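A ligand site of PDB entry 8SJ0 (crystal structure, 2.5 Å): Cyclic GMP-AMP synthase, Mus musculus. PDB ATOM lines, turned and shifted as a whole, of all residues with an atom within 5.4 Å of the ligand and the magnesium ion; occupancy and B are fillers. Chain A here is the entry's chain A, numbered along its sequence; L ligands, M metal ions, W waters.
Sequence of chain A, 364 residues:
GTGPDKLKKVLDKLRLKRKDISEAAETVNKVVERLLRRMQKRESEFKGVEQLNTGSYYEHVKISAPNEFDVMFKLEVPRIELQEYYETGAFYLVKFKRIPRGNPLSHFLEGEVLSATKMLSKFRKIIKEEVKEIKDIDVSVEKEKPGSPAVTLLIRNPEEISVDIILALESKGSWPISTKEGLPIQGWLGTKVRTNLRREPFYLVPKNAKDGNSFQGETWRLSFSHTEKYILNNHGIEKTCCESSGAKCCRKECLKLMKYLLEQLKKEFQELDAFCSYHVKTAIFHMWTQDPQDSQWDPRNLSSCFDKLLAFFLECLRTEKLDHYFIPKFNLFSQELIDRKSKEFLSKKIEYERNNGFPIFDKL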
ATOM      1  N   THR A  54     -30.936  -3.638  17.257  1.00  0.00           N
ATOM      2  CA  THR A  54     -29.610  -4.217  16.987  1.00  0.00           C
ATOM      3  C   THR A  54     -29.142  -3.851  15.582  1.00  0.00           C
ATOM      4  O   THR A  54     -29.875  -3.240  14.786  1.00  0.00           O
ATOM      5  CB  THR A  54     -29.640  -5.741  17.098  1.00  0.00           C
ATOM      6  OG1 THR A  54     -30.431  -6.259  16.025  1.00  0.00           O
ATOM      7  CG2 THR A  54     -30.255  -6.158  18.375  1.00  0.00           C
ATOM      8  N   GLY A  55     -27.921  -4.262  15.247  1.00  0.00           N
ATOM      9  CA  GLY A  55     -27.500  -4.135  13.867  1.00  0.00           C
ATOM     10  C   GLY A  55     -26.903  -2.777  13.534  1.00  0.00           C
ATOM     11  O   GLY A  55     -26.736  -1.883  14.378  1.00  0.00           O
ATOM     12  N   SER A  56     -26.583  -2.624  12.253  1.00  0.00           N
ATOM     13  CA  SER A  56     -25.601  -1.619  11.892  1.00  0.00           C
ATOM     14  C   SER A  56     -26.163  -0.209  12.003  1.00  0.00           C
ATOM     15  O   SER A  56     -25.404   0.730  12.241  1.00  0.00           O
ATOM     16  CB  SER A  56     -25.063  -1.899  10.502  1.00  0.00           C
ATOM     17  OG  SER A  56     -25.974  -1.431   9.522  1.00  0.00           O
ATOM     18  N   TYR A  57     -27.492  -0.044  11.863  1.00  0.00           N
ATOM     19  CA  TYR A  57     -28.073   1.302  11.966  1.00  0.00           C
ATOM     20  C   TYR A  57     -28.001   1.835  13.391  1.00  0.00           C
ATOM     21  O   TYR A  57     -27.825   3.045  13.602  1.00  0.00           O
ATOM     22  CB  TYR A  57     -29.516   1.304  11.481  1.00  0.00           C
ATOM     23  CG  TYR A  57     -30.279   2.559  11.871  1.00  0.00           C
ATOM     24  CD1 TYR A  57     -30.215   3.704  11.078  1.00  0.00           C
ATOM     25  CD2 TYR A  57     -31.065   2.588  13.022  1.00  0.00           C
ATOM     26  CE1 TYR A  57     -30.915   4.865  11.424  1.00  0.00           C
ATOM     27  CE2 TYR A  57     -31.781   3.726  13.369  1.00  0.00           C
ATOM     28  CZ  TYR A  57     -31.684   4.866  12.571  1.00  0.00           C
ATOM     29  OH  TYR A  57     -32.374   6.020  12.910  1.00  0.00           O
ATOM     30  N   GLU A  59     -25.707   0.595  15.581  1.00  0.00           N
ATOM     31  CA  GLU A  59     -24.273   0.711  15.784  1.00  0.00           C
ATOM     32  C   GLU A  59     -23.676   1.923  15.068  1.00  0.00           C
ATOM     33  O   GLU A  59     -22.526   2.269  15.355  1.00  0.00           O
ATOM     34  CB  GLU A  59     -23.569  -0.574  15.333  1.00  0.00           C
ATOM     35  CG  GLU A  59     -23.878  -1.836  16.185  1.00  0.00           C
ATOM     36  CD  GLU A  59     -23.649  -3.140  15.416  1.00  0.00           C
ATOM     37  OE1 GLU A  59     -23.264  -3.061  14.221  1.00  0.00           O
ATOM     38  OE2 GLU A  59     -23.850  -4.252  15.997  1.00  0.00           O
ATOM     39  N   VAL A  61     -23.093   2.162  11.752  1.00  0.00           N
ATOM     40  CA  VAL A  61     -22.256   1.736  10.625  1.00  0.00           C
ATOM     41  C   VAL A  61     -23.148   1.350   9.442  1.00  0.00           C
ATOM     42  O   VAL A  61     -22.724   0.633   8.530  1.00  0.00           O
ATOM     43  CB  VAL A  61     -21.305   0.583  11.007  1.00  0.00           C
ATOM     44  CG1 VAL A  61     -20.229   1.054  11.956  1.00  0.00           C
ATOM     45  CG2 VAL A  61     -22.045  -0.607  11.602  1.00  0.00           C
ATOM     46  N   LYS A  62     -24.399   1.805   9.450  1.00  0.00           N
ATOM     47  CA  LYS A  62     -25.251   1.664   8.283  1.00  0.00           C
ATOM     48  C   LYS A  62     -24.755   2.612   7.211  1.00  0.00           C
ATOM     49  O   LYS A  62     -24.523   3.795   7.490  1.00  0.00           O
ATOM     50  CB  LYS A  62     -26.694   1.967   8.657  1.00  0.00           C
ATOM     51  CG  LYS A  62     -27.686   1.827   7.556  1.00  0.00           C
ATOM     52  CD  LYS A  62     -27.713   0.426   7.028  1.00  0.00           C
ATOM     53  CE  LYS A  62     -28.681   0.378   5.885  1.00  0.00           C
ATOM     54  NZ  LYS A  62     -28.126  -0.263   4.682  1.00  0.00           N
ATOM     55  N   GLU A  68     -32.517  -0.253   5.980  1.00  0.00           N
ATOM     56  CA  GLU A  68     -32.582  -1.607   6.543  1.00  0.00           C
ATOM     57  C   GLU A  68     -32.381  -1.520   8.046  1.00  0.00           C
ATOM     58  O   GLU A  68     -31.281  -1.205   8.496  1.00  0.00           O
ATOM     59  CB  GLU A  68     -31.526  -2.510   5.898  1.00  0.00           C
ATOM     60  CG  GLU A  68     -31.814  -4.002   5.968  1.00  0.00           C
ATOM     61  CD  GLU A  68     -31.367  -4.631   7.292  1.00  0.00           C
ATOM     62  OE1 GLU A  68     -30.552  -4.012   8.017  1.00  0.00           O
ATOM     63  OE2 GLU A  68     -31.811  -5.769   7.603  1.00  0.00           O
ATOM     64  N   PHE A  69     -33.433  -1.842   8.813  1.00  0.00           N
ATOM     65  CA  PHE A  69     -33.455  -1.780  10.265  1.00  0.00           C
ATOM     66  C   PHE A  69     -33.599  -3.175  10.854  1.00  0.00           C
ATOM     67  O   PHE A  69     -34.337  -4.008  10.317  1.00  0.00           O
ATOM     68  CB  PHE A  69     -34.637  -0.917  10.730  1.00  0.00           C
ATOM     69  CG  PHE A  69     -34.535   0.527  10.324  1.00  0.00           C
ATOM     70  CD1 PHE A  69     -34.776   0.911   9.017  1.00  0.00           C
ATOM     71  CD2 PHE A  69     -34.180   1.494  11.248  1.00  0.00           C
ATOM     72  CE1 PHE A  69     -34.678   2.248   8.639  1.00  0.00           C
ATOM     73  CE2 PHE A  69     -34.064   2.820  10.881  1.00  0.00           C
ATOM     74  CZ  PHE A  69     -34.321   3.190   9.579  1.00  0.00           C
ATOM     75  N   ASP A  70     -32.909  -3.453  11.968  1.00  0.00           N
ATOM     76  CA  ASP A  70     -32.979  -4.768  12.601  1.00  0.00           C
ATOM     77  C   ASP A  70     -33.411  -4.632  14.049  1.00  0.00           C
ATOM     78  O   ASP A  70     -32.840  -3.819  14.795  1.00  0.00           O
ATOM     79  CB  ASP A  70     -31.639  -5.486  12.524  1.00  0.00           C
ATOM     80  CG  ASP A  70     -31.163  -5.667  11.099  1.00  0.00           C
ATOM     81  OD1 ASP A  70     -31.916  -6.253  10.274  1.00  0.00           O
ATOM     82  OD2 ASP A  70     -30.034  -5.231  10.806  1.00  0.00           O
ATOM     83  N   ASP A 164     -36.095  -6.247   9.683  1.00  0.00           N
ATOM     84  CA  ASP A 164     -36.037  -7.625  10.147  1.00  0.00           C
ATOM     85  C   ASP A 164     -36.504  -7.669  11.607  1.00  0.00           C
ATOM     86  O   ASP A 164     -35.828  -7.123  12.491  1.00  0.00           O
ATOM     87  CB  ASP A 164     -34.611  -8.156  10.025  1.00  0.00           C
ATOM     88  CG  ASP A 164     -34.257  -8.553   8.620  1.00  0.00           C
ATOM     89  OD1 ASP A 164     -35.189  -8.607   7.789  1.00  0.00           O
ATOM     90  OD2 ASP A 164     -33.078  -8.816   8.336  1.00  0.00           O
ATOM     91  N   ILE A 166     -36.634  -9.965  14.512  1.00  0.00           N
ATOM     92  CA  ILE A 166     -35.995 -11.210  14.912  1.00  0.00           C
ATOM     93  C   ILE A 166     -36.640 -11.700  16.205  1.00  0.00           C
ATOM     94  O   ILE A 166     -36.831 -10.940  17.146  1.00  0.00           O
ATOM     95  CB  ILE A 166     -34.476 -11.008  15.054  1.00  0.00           C
ATOM     96  CG1 ILE A 166     -33.909 -10.417  13.746  1.00  0.00           C
ATOM     97  CG2 ILE A 166     -33.786 -12.295  15.441  1.00  0.00           C
ATOM     98  CD1 ILE A 166     -32.919  -9.217  13.937  1.00  0.00           C
ATOM     99  N   ARG A 221     -30.071 -20.950  17.589  1.00  0.00           N
ATOM    100  CA  ARG A 221     -28.758 -20.380  17.292  1.00  0.00           C
ATOM    101  C   ARG A 221     -28.437 -19.270  18.284  1.00  0.00           C
ATOM    102  O   ARG A 221     -29.288 -18.418  18.569  1.00  0.00           O
ATOM    103  CB  ARG A 221     -28.755 -19.847  15.834  1.00  0.00           C
ATOM    104  CG  ARG A 221     -27.415 -19.370  15.259  1.00  0.00           C
ATOM    105  CD  ARG A 221     -27.634 -18.749  13.861  1.00  0.00           C
ATOM    106  NE  ARG A 221     -27.870 -17.314  13.998  1.00  0.00           N
ATOM    107  CZ  ARG A 221     -28.836 -16.648  13.383  1.00  0.00           C
ATOM    108  NH1 ARG A 221     -29.647 -17.239  12.516  1.00  0.00           N
ATOM    109  NH2 ARG A 221     -28.991 -15.346  13.661  1.00  0.00           N
ATOM    110  N   LEU A 222     -27.218 -19.284  18.837  1.00  0.00           N
ATOM    111  CA  LEU A 222     -26.828 -18.229  19.770  1.00  0.00           C
ATOM    112  C   LEU A 222     -26.699 -16.896  19.046  1.00  0.00           C
ATOM    113  O   LEU A 222     -26.188 -16.838  17.933  1.00  0.00           O
ATOM    114  CB  LEU A 222     -25.497 -18.566  20.442  1.00  0.00           C
ATOM    115  CG  LEU A 222     -25.483 -19.628  21.551  1.00  0.00           C
ATOM    116  CD1 LEU A 222     -24.079 -19.969  21.982  1.00  0.00           C
ATOM    117  CD2 LEU A 222     -26.293 -19.158  22.746  1.00  0.00           C
ATOM    118  N   GLU A 228     -22.526  -7.124  20.656  1.00  0.00           N
ATOM    119  CA  GLU A 228     -21.910  -6.450  19.530  1.00  0.00           C
ATOM    120  C   GLU A 228     -22.286  -4.971  19.483  1.00  0.00           C
ATOM    121  O   GLU A 228     -21.466  -4.123  19.108  1.00  0.00           O
ATOM    122  CB  GLU A 228     -22.299  -7.177  18.233  1.00  0.00           C
ATOM    123  CG  GLU A 228     -21.905  -8.677  18.256  1.00  0.00           C
ATOM    124  CD  GLU A 228     -22.463  -9.477  17.074  1.00  0.00           C
ATOM    125  OE1 GLU A 228     -22.987  -8.872  16.099  1.00  0.00           O
ATOM    126  OE2 GLU A 228     -22.360 -10.726  17.120  1.00  0.00           O
ATOM    127  N   LYS A 259     -17.659  -3.043   4.580  1.00  0.00           N
ATOM    128  CA  LYS A 259     -19.040  -3.423   4.300  1.00  0.00           C
ATOM    129  C   LYS A 259     -19.439  -3.047   2.895  1.00  0.00           C
ATOM    130  O   LYS A 259     -20.112  -3.826   2.195  1.00  0.00           O
ATOM    131  CB  LYS A 259     -19.989  -2.741   5.289  1.00  0.00           C
ATOM    132  CG  LYS A 259     -20.025  -3.331   6.680  1.00  0.00           C
ATOM    133  CD  LYS A 259     -20.482  -2.278   7.655  1.00  0.00           C
ATOM    134  CE  LYS A 259     -21.915  -1.855   7.375  1.00  0.00           C
ATOM    135  NZ  LYS A 259     -22.875  -2.861   7.874  1.00  0.00           N
ATOM    136  N   GLU A 263     -20.668  -5.157  -0.139  1.00  0.00           N
ATOM    137  CA  GLU A 263     -22.003  -4.838  -0.666  1.00  0.00           C
ATOM    138  C   GLU A 263     -21.983  -4.639  -2.169  1.00  0.00           C
ATOM    139  O   GLU A 263     -22.810  -5.182  -2.901  1.00  0.00           O
ATOM    140  CB  GLU A 263     -22.559  -3.585   0.026  1.00  0.00           C
ATOM    141  CG  GLU A 263     -23.857  -3.755   0.780  1.00  0.00           C
ATOM    142  CD  GLU A 263     -24.297  -2.482   1.525  1.00  0.00           C
ATOM    143  OE1 GLU A 263     -24.543  -1.435   0.863  1.00  0.00           O
ATOM    144  OE2 GLU A 263     -24.394  -2.512   2.782  1.00  0.00           O
ATOM    145  N   CYS A 276     -21.732 -12.330   3.616  1.00  0.00           N
ATOM    146  CA  CYS A 276     -22.638 -11.391   4.247  1.00  0.00           C
ATOM    147  C   CYS A 276     -21.826 -10.494   5.154  1.00  0.00           C
ATOM    148  O   CYS A 276     -20.700 -10.824   5.537  1.00  0.00           O
ATOM    149  CB  CYS A 276     -23.755 -12.110   5.025  1.00  0.00           C
ATOM    150  SG  CYS A 276     -23.167 -13.022   6.454  1.00  0.00           S
ATOM    151  N   SER A 277     -22.425  -9.366   5.511  1.00  0.00           N
ATOM    152  CA  SER A 277     -21.709  -8.368   6.275  1.00  0.00           C
ATOM    153  C   SER A 277     -21.233  -8.905   7.622  1.00  0.00           C
ATOM    154  O   SER A 277     -20.252  -8.408   8.179  1.00  0.00           O
ATOM    155  CB  SER A 277     -22.584  -7.147   6.469  1.00  0.00           C
ATOM    156  OG  SER A 277     -23.769  -7.574   7.053  1.00  0.00           O
ATOM    157  N   TYR A 278     -21.910  -9.927   8.155  1.00  0.00           N
ATOM    158  CA  TYR A 278     -21.440 -10.480   9.420  1.00  0.00           C
ATOM    159  C   TYR A 278     -20.030 -11.043   9.263  1.00  0.00           C
ATOM    160  O   TYR A 278     -19.242 -11.043  10.226  1.00  0.00           O
ATOM    161  CB  TYR A 278     -22.408 -11.548   9.940  1.00  0.00           C
ATOM    162  CG  TYR A 278     -22.139 -11.854  11.403  1.00  0.00           C
ATOM    163  CD1 TYR A 278     -22.394 -10.900  12.371  1.00  0.00           C
ATOM    164  CD2 TYR A 278     -21.574 -13.075  11.799  1.00  0.00           C
ATOM    165  CE1 TYR A 278     -22.135 -11.143  13.708  1.00  0.00           C
ATOM    166  CE2 TYR A 278     -21.287 -13.328  13.143  1.00  0.00           C
ATOM    167  CZ  TYR A 278     -21.579 -12.359  14.087  1.00  0.00           C
ATOM    168  OH  TYR A 278     -21.339 -12.556  15.435  1.00  0.00           O
ATOM    169  N   LYS A 281     -17.857  -8.092   9.697  1.00  0.00           N
ATOM    170  CA  LYS A 281     -17.938  -7.621  11.086  1.00  0.00           C
ATOM    171  C   LYS A 281     -17.097  -8.485  12.010  1.00  0.00           C
ATOM    172  O   LYS A 281     -16.465  -7.986  12.948  1.00  0.00           O
ATOM    173  CB  LYS A 281     -19.375  -7.606  11.558  1.00  0.00           C
ATOM    174  CG  LYS A 281     -19.586  -6.925  12.873  1.00  0.00           C
ATOM    175  CD  LYS A 281     -20.940  -7.275  13.444  1.00  0.00           C
ATOM    176  CE  LYS A 281     -21.506  -6.114  14.217  1.00  0.00           C
ATOM    177  NZ  LYS A 281     -22.813  -6.450  14.861  1.00  0.00           N
ATOM    178  N   HIS A 324     -15.889 -17.556  14.682  1.00  0.00           N
ATOM    179  CA  HIS A 324     -16.847 -16.707  15.368  1.00  0.00           C
ATOM    180  C   HIS A 324     -16.211 -16.018  16.562  1.00  0.00           C
ATOM    181  O   HIS A 324     -15.515 -16.655  17.356  1.00  0.00           O
ATOM    182  CB  HIS A 324     -18.048 -17.549  15.821  1.00  0.00           C
ATOM    183  CG  HIS A 324     -19.269 -16.741  16.118  1.00  0.00           C
ATOM    184  ND1 HIS A 324     -19.448 -16.068  17.314  1.00  0.00           N
ATOM    185  CD2 HIS A 324     -20.401 -16.544  15.405  1.00  0.00           C
ATOM    186  CE1 HIS A 324     -20.631 -15.479  17.304  1.00  0.00           C
ATOM    187  NE2 HIS A 324     -21.227 -15.754  16.162  1.00  0.00           N
HETATM  188  P1  LIG L   1     -26.119  -4.444   7.436  1.00  0.00           P
HETATM  189  O1  LIG L   1     -25.718  -5.172   6.178  1.00  0.00           O
HETATM  190  O2  LIG L   1     -25.564  -3.013   7.497  1.00  0.00           O
HETATM  191  O3  LIG L   1     -27.698  -4.392   7.712  1.00  0.00           O
HETATM  192  P2  LIG L   1     -26.015  -5.653  10.250  1.00  0.00           P
HETATM  193  O4  LIG L   1     -24.939  -5.780  11.294  1.00  0.00           O
HETATM  194  O5  LIG L   1     -27.228  -4.757  10.603  1.00  0.00           O
HETATM  195  O6  LIG L   1     -25.510  -5.187   8.754  1.00  0.00           O
HETATM  196  P3  LIG L   1     -28.023  -7.711   9.670  1.00  0.00           P
HETATM  197  O7  LIG L   1     -28.854  -6.713   8.949  1.00  0.00           O
HETATM  198  O8  LIG L   1     -28.599  -8.262  10.982  1.00  0.00           O
HETATM  199  O9  LIG L   1     -26.610  -7.097   9.966  1.00  0.00           O
HETATM  200  O10 LIG L   1     -27.584  -8.903   8.721  1.00  0.00           O
HETATM  201  C1  LIG L   1     -26.610  -8.707   7.669  1.00  0.00           C
HETATM  202  C2  LIG L   1     -26.327 -10.042   7.015  1.00  0.00           C
HETATM  203  O11 LIG L   1     -25.571 -10.815   7.982  1.00  0.00           O
HETATM  204  C3  LIG L   1     -27.652 -10.786   6.824  1.00  0.00           C
HETATM  205  O12 LIG L   1     -27.533 -11.671   5.723  1.00  0.00           O
HETATM  206  C4  LIG L   1     -27.753 -11.641   8.090  1.00  0.00           C
HETATM  207  C5  LIG L   1     -26.293 -11.963   8.398  1.00  0.00           C
HETATM  208  N1  LIG L   1     -26.058 -12.095   9.835  1.00  0.00           N
HETATM  209  C6  LIG L   1     -26.215 -11.138  10.803  1.00  0.00           C
HETATM  210  N2  LIG L   1     -25.915 -11.546  12.017  1.00  0.00           N
HETATM  211  C7  LIG L   1     -25.529 -12.869  11.831  1.00  0.00           C
HETATM  212  C8  LIG L   1     -25.068 -13.857  12.717  1.00  0.00           C
HETATM  213  N3  LIG L   1     -24.942 -13.667  14.044  1.00  0.00           N
HETATM  214  N4  LIG L   1     -24.750 -15.077  12.204  1.00  0.00           N
HETATM  215  C9  LIG L   1     -24.881 -15.272  10.889  1.00  0.00           C
HETATM  216  N5  LIG L   1     -25.288 -14.405   9.944  1.00  0.00           N
HETATM  217  C10 LIG L   1     -25.605 -13.219  10.493  1.00  0.00           C
HETATM  218 MG    MG M   1     -28.688  -2.803   9.396  1.00  0.00          MG
HETATM  219  O   HOH W   1     -30.334  -2.152  12.059  1.00  0.00           O
HETATM  220  O   HOH W   2     -23.284  -4.034  11.805  1.00  0.00           O
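An oxygen (O2) of the ligand is in salt-bridge range of the side-chain amino group (NZ) of Lys 259, at 2.7 Å.
The side-chain carboxylate (OD2) of Asp 70 sits close to an oxygen (O7) of the ligand (2.7 Å).
N of Ser 56 lies within hydrogen-bond range of O5 of the ligand, at 2.8 Å.
An oxygen (O1) of the ligand lies close to the side-chain hydroxyl (OG) of Ser 277 (3.2 Å).
O2 of the ligand lies within hydrogen-bond range of OG of Ser 56 (2.6 Å).
O11 of the ligand is in hydrogen-bond range of SG of Cys 276, 3.6 Å away.
The backbone NH of Lys 62 is in hydrogen-bond range of the backbone carbonyl oxygen of Ser 56 (3.2 Å).
OH of Tyr 278 lies within hydrogen-bond range of OE2 of Glu 228, at 2.7 Å.
The backbone NH (N) of Thr 54 is in hydrogen-bond range of the backbone carbonyl oxygen (O) of Asp 70 (3.1 Å).
A ring nitrogen (NE2) of His 324 lies within hydrogen-bond range of the side-chain hydroxyl of Tyr 278, 3.3 Å away.
O of Ser 56 is in hydrogen-bond range of N of Val 61 (2.8 Å).
The side-chain carboxylate (OD1) of Asp 70 sits close to the side-chain carboxylate (OE2) of Glu 68 (2.7 Å).
The side-chain sulfur (SG) of Cys 276 sits close to the backbone NH (N) of Tyr 278 (3.7 Å).
Gly 55 touches the ligand (CA to O5, 3.3 Å).
Tyr 278 touches the ligand (CG to C7, 3.6 Å).
Hydrophobic or aromatic side chains that line the ligand: Tyr 278.
OG of Ser 56 touches the magnesium ion (3.0 Å).
Tyr 57 touches the magnesium ion (N to MG, 3.9 Å).
Asp 70 touches the magnesium ion (OD2 to MG, 3.1 Å).
Within 4 Å of the magnesium ion: Ser 56, Tyr 57, Glu 68 and Asp 70.
The nearest printed residue that does not touch the magnesium ion is Lys 62 (4.1 Å).
The magnesium ion is bound by an oxygen (O3) of the ligand (2.5 Å).
Slightly farther from the magnesium ion lies the side-chain carboxylate (OE1) of Glu 68 (2.6 Å).
Slightly farther from the magnesium ion lies O5 of the ligand (2.7 Å).
Water W2 bridges O4 of the ligand (2.5 Å) and OE1 of Glu 59 (2.6 Å).
Water W1 bridges N of Asp 70 (2.9 Å) and O of Thr 54 (3.0 Å).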
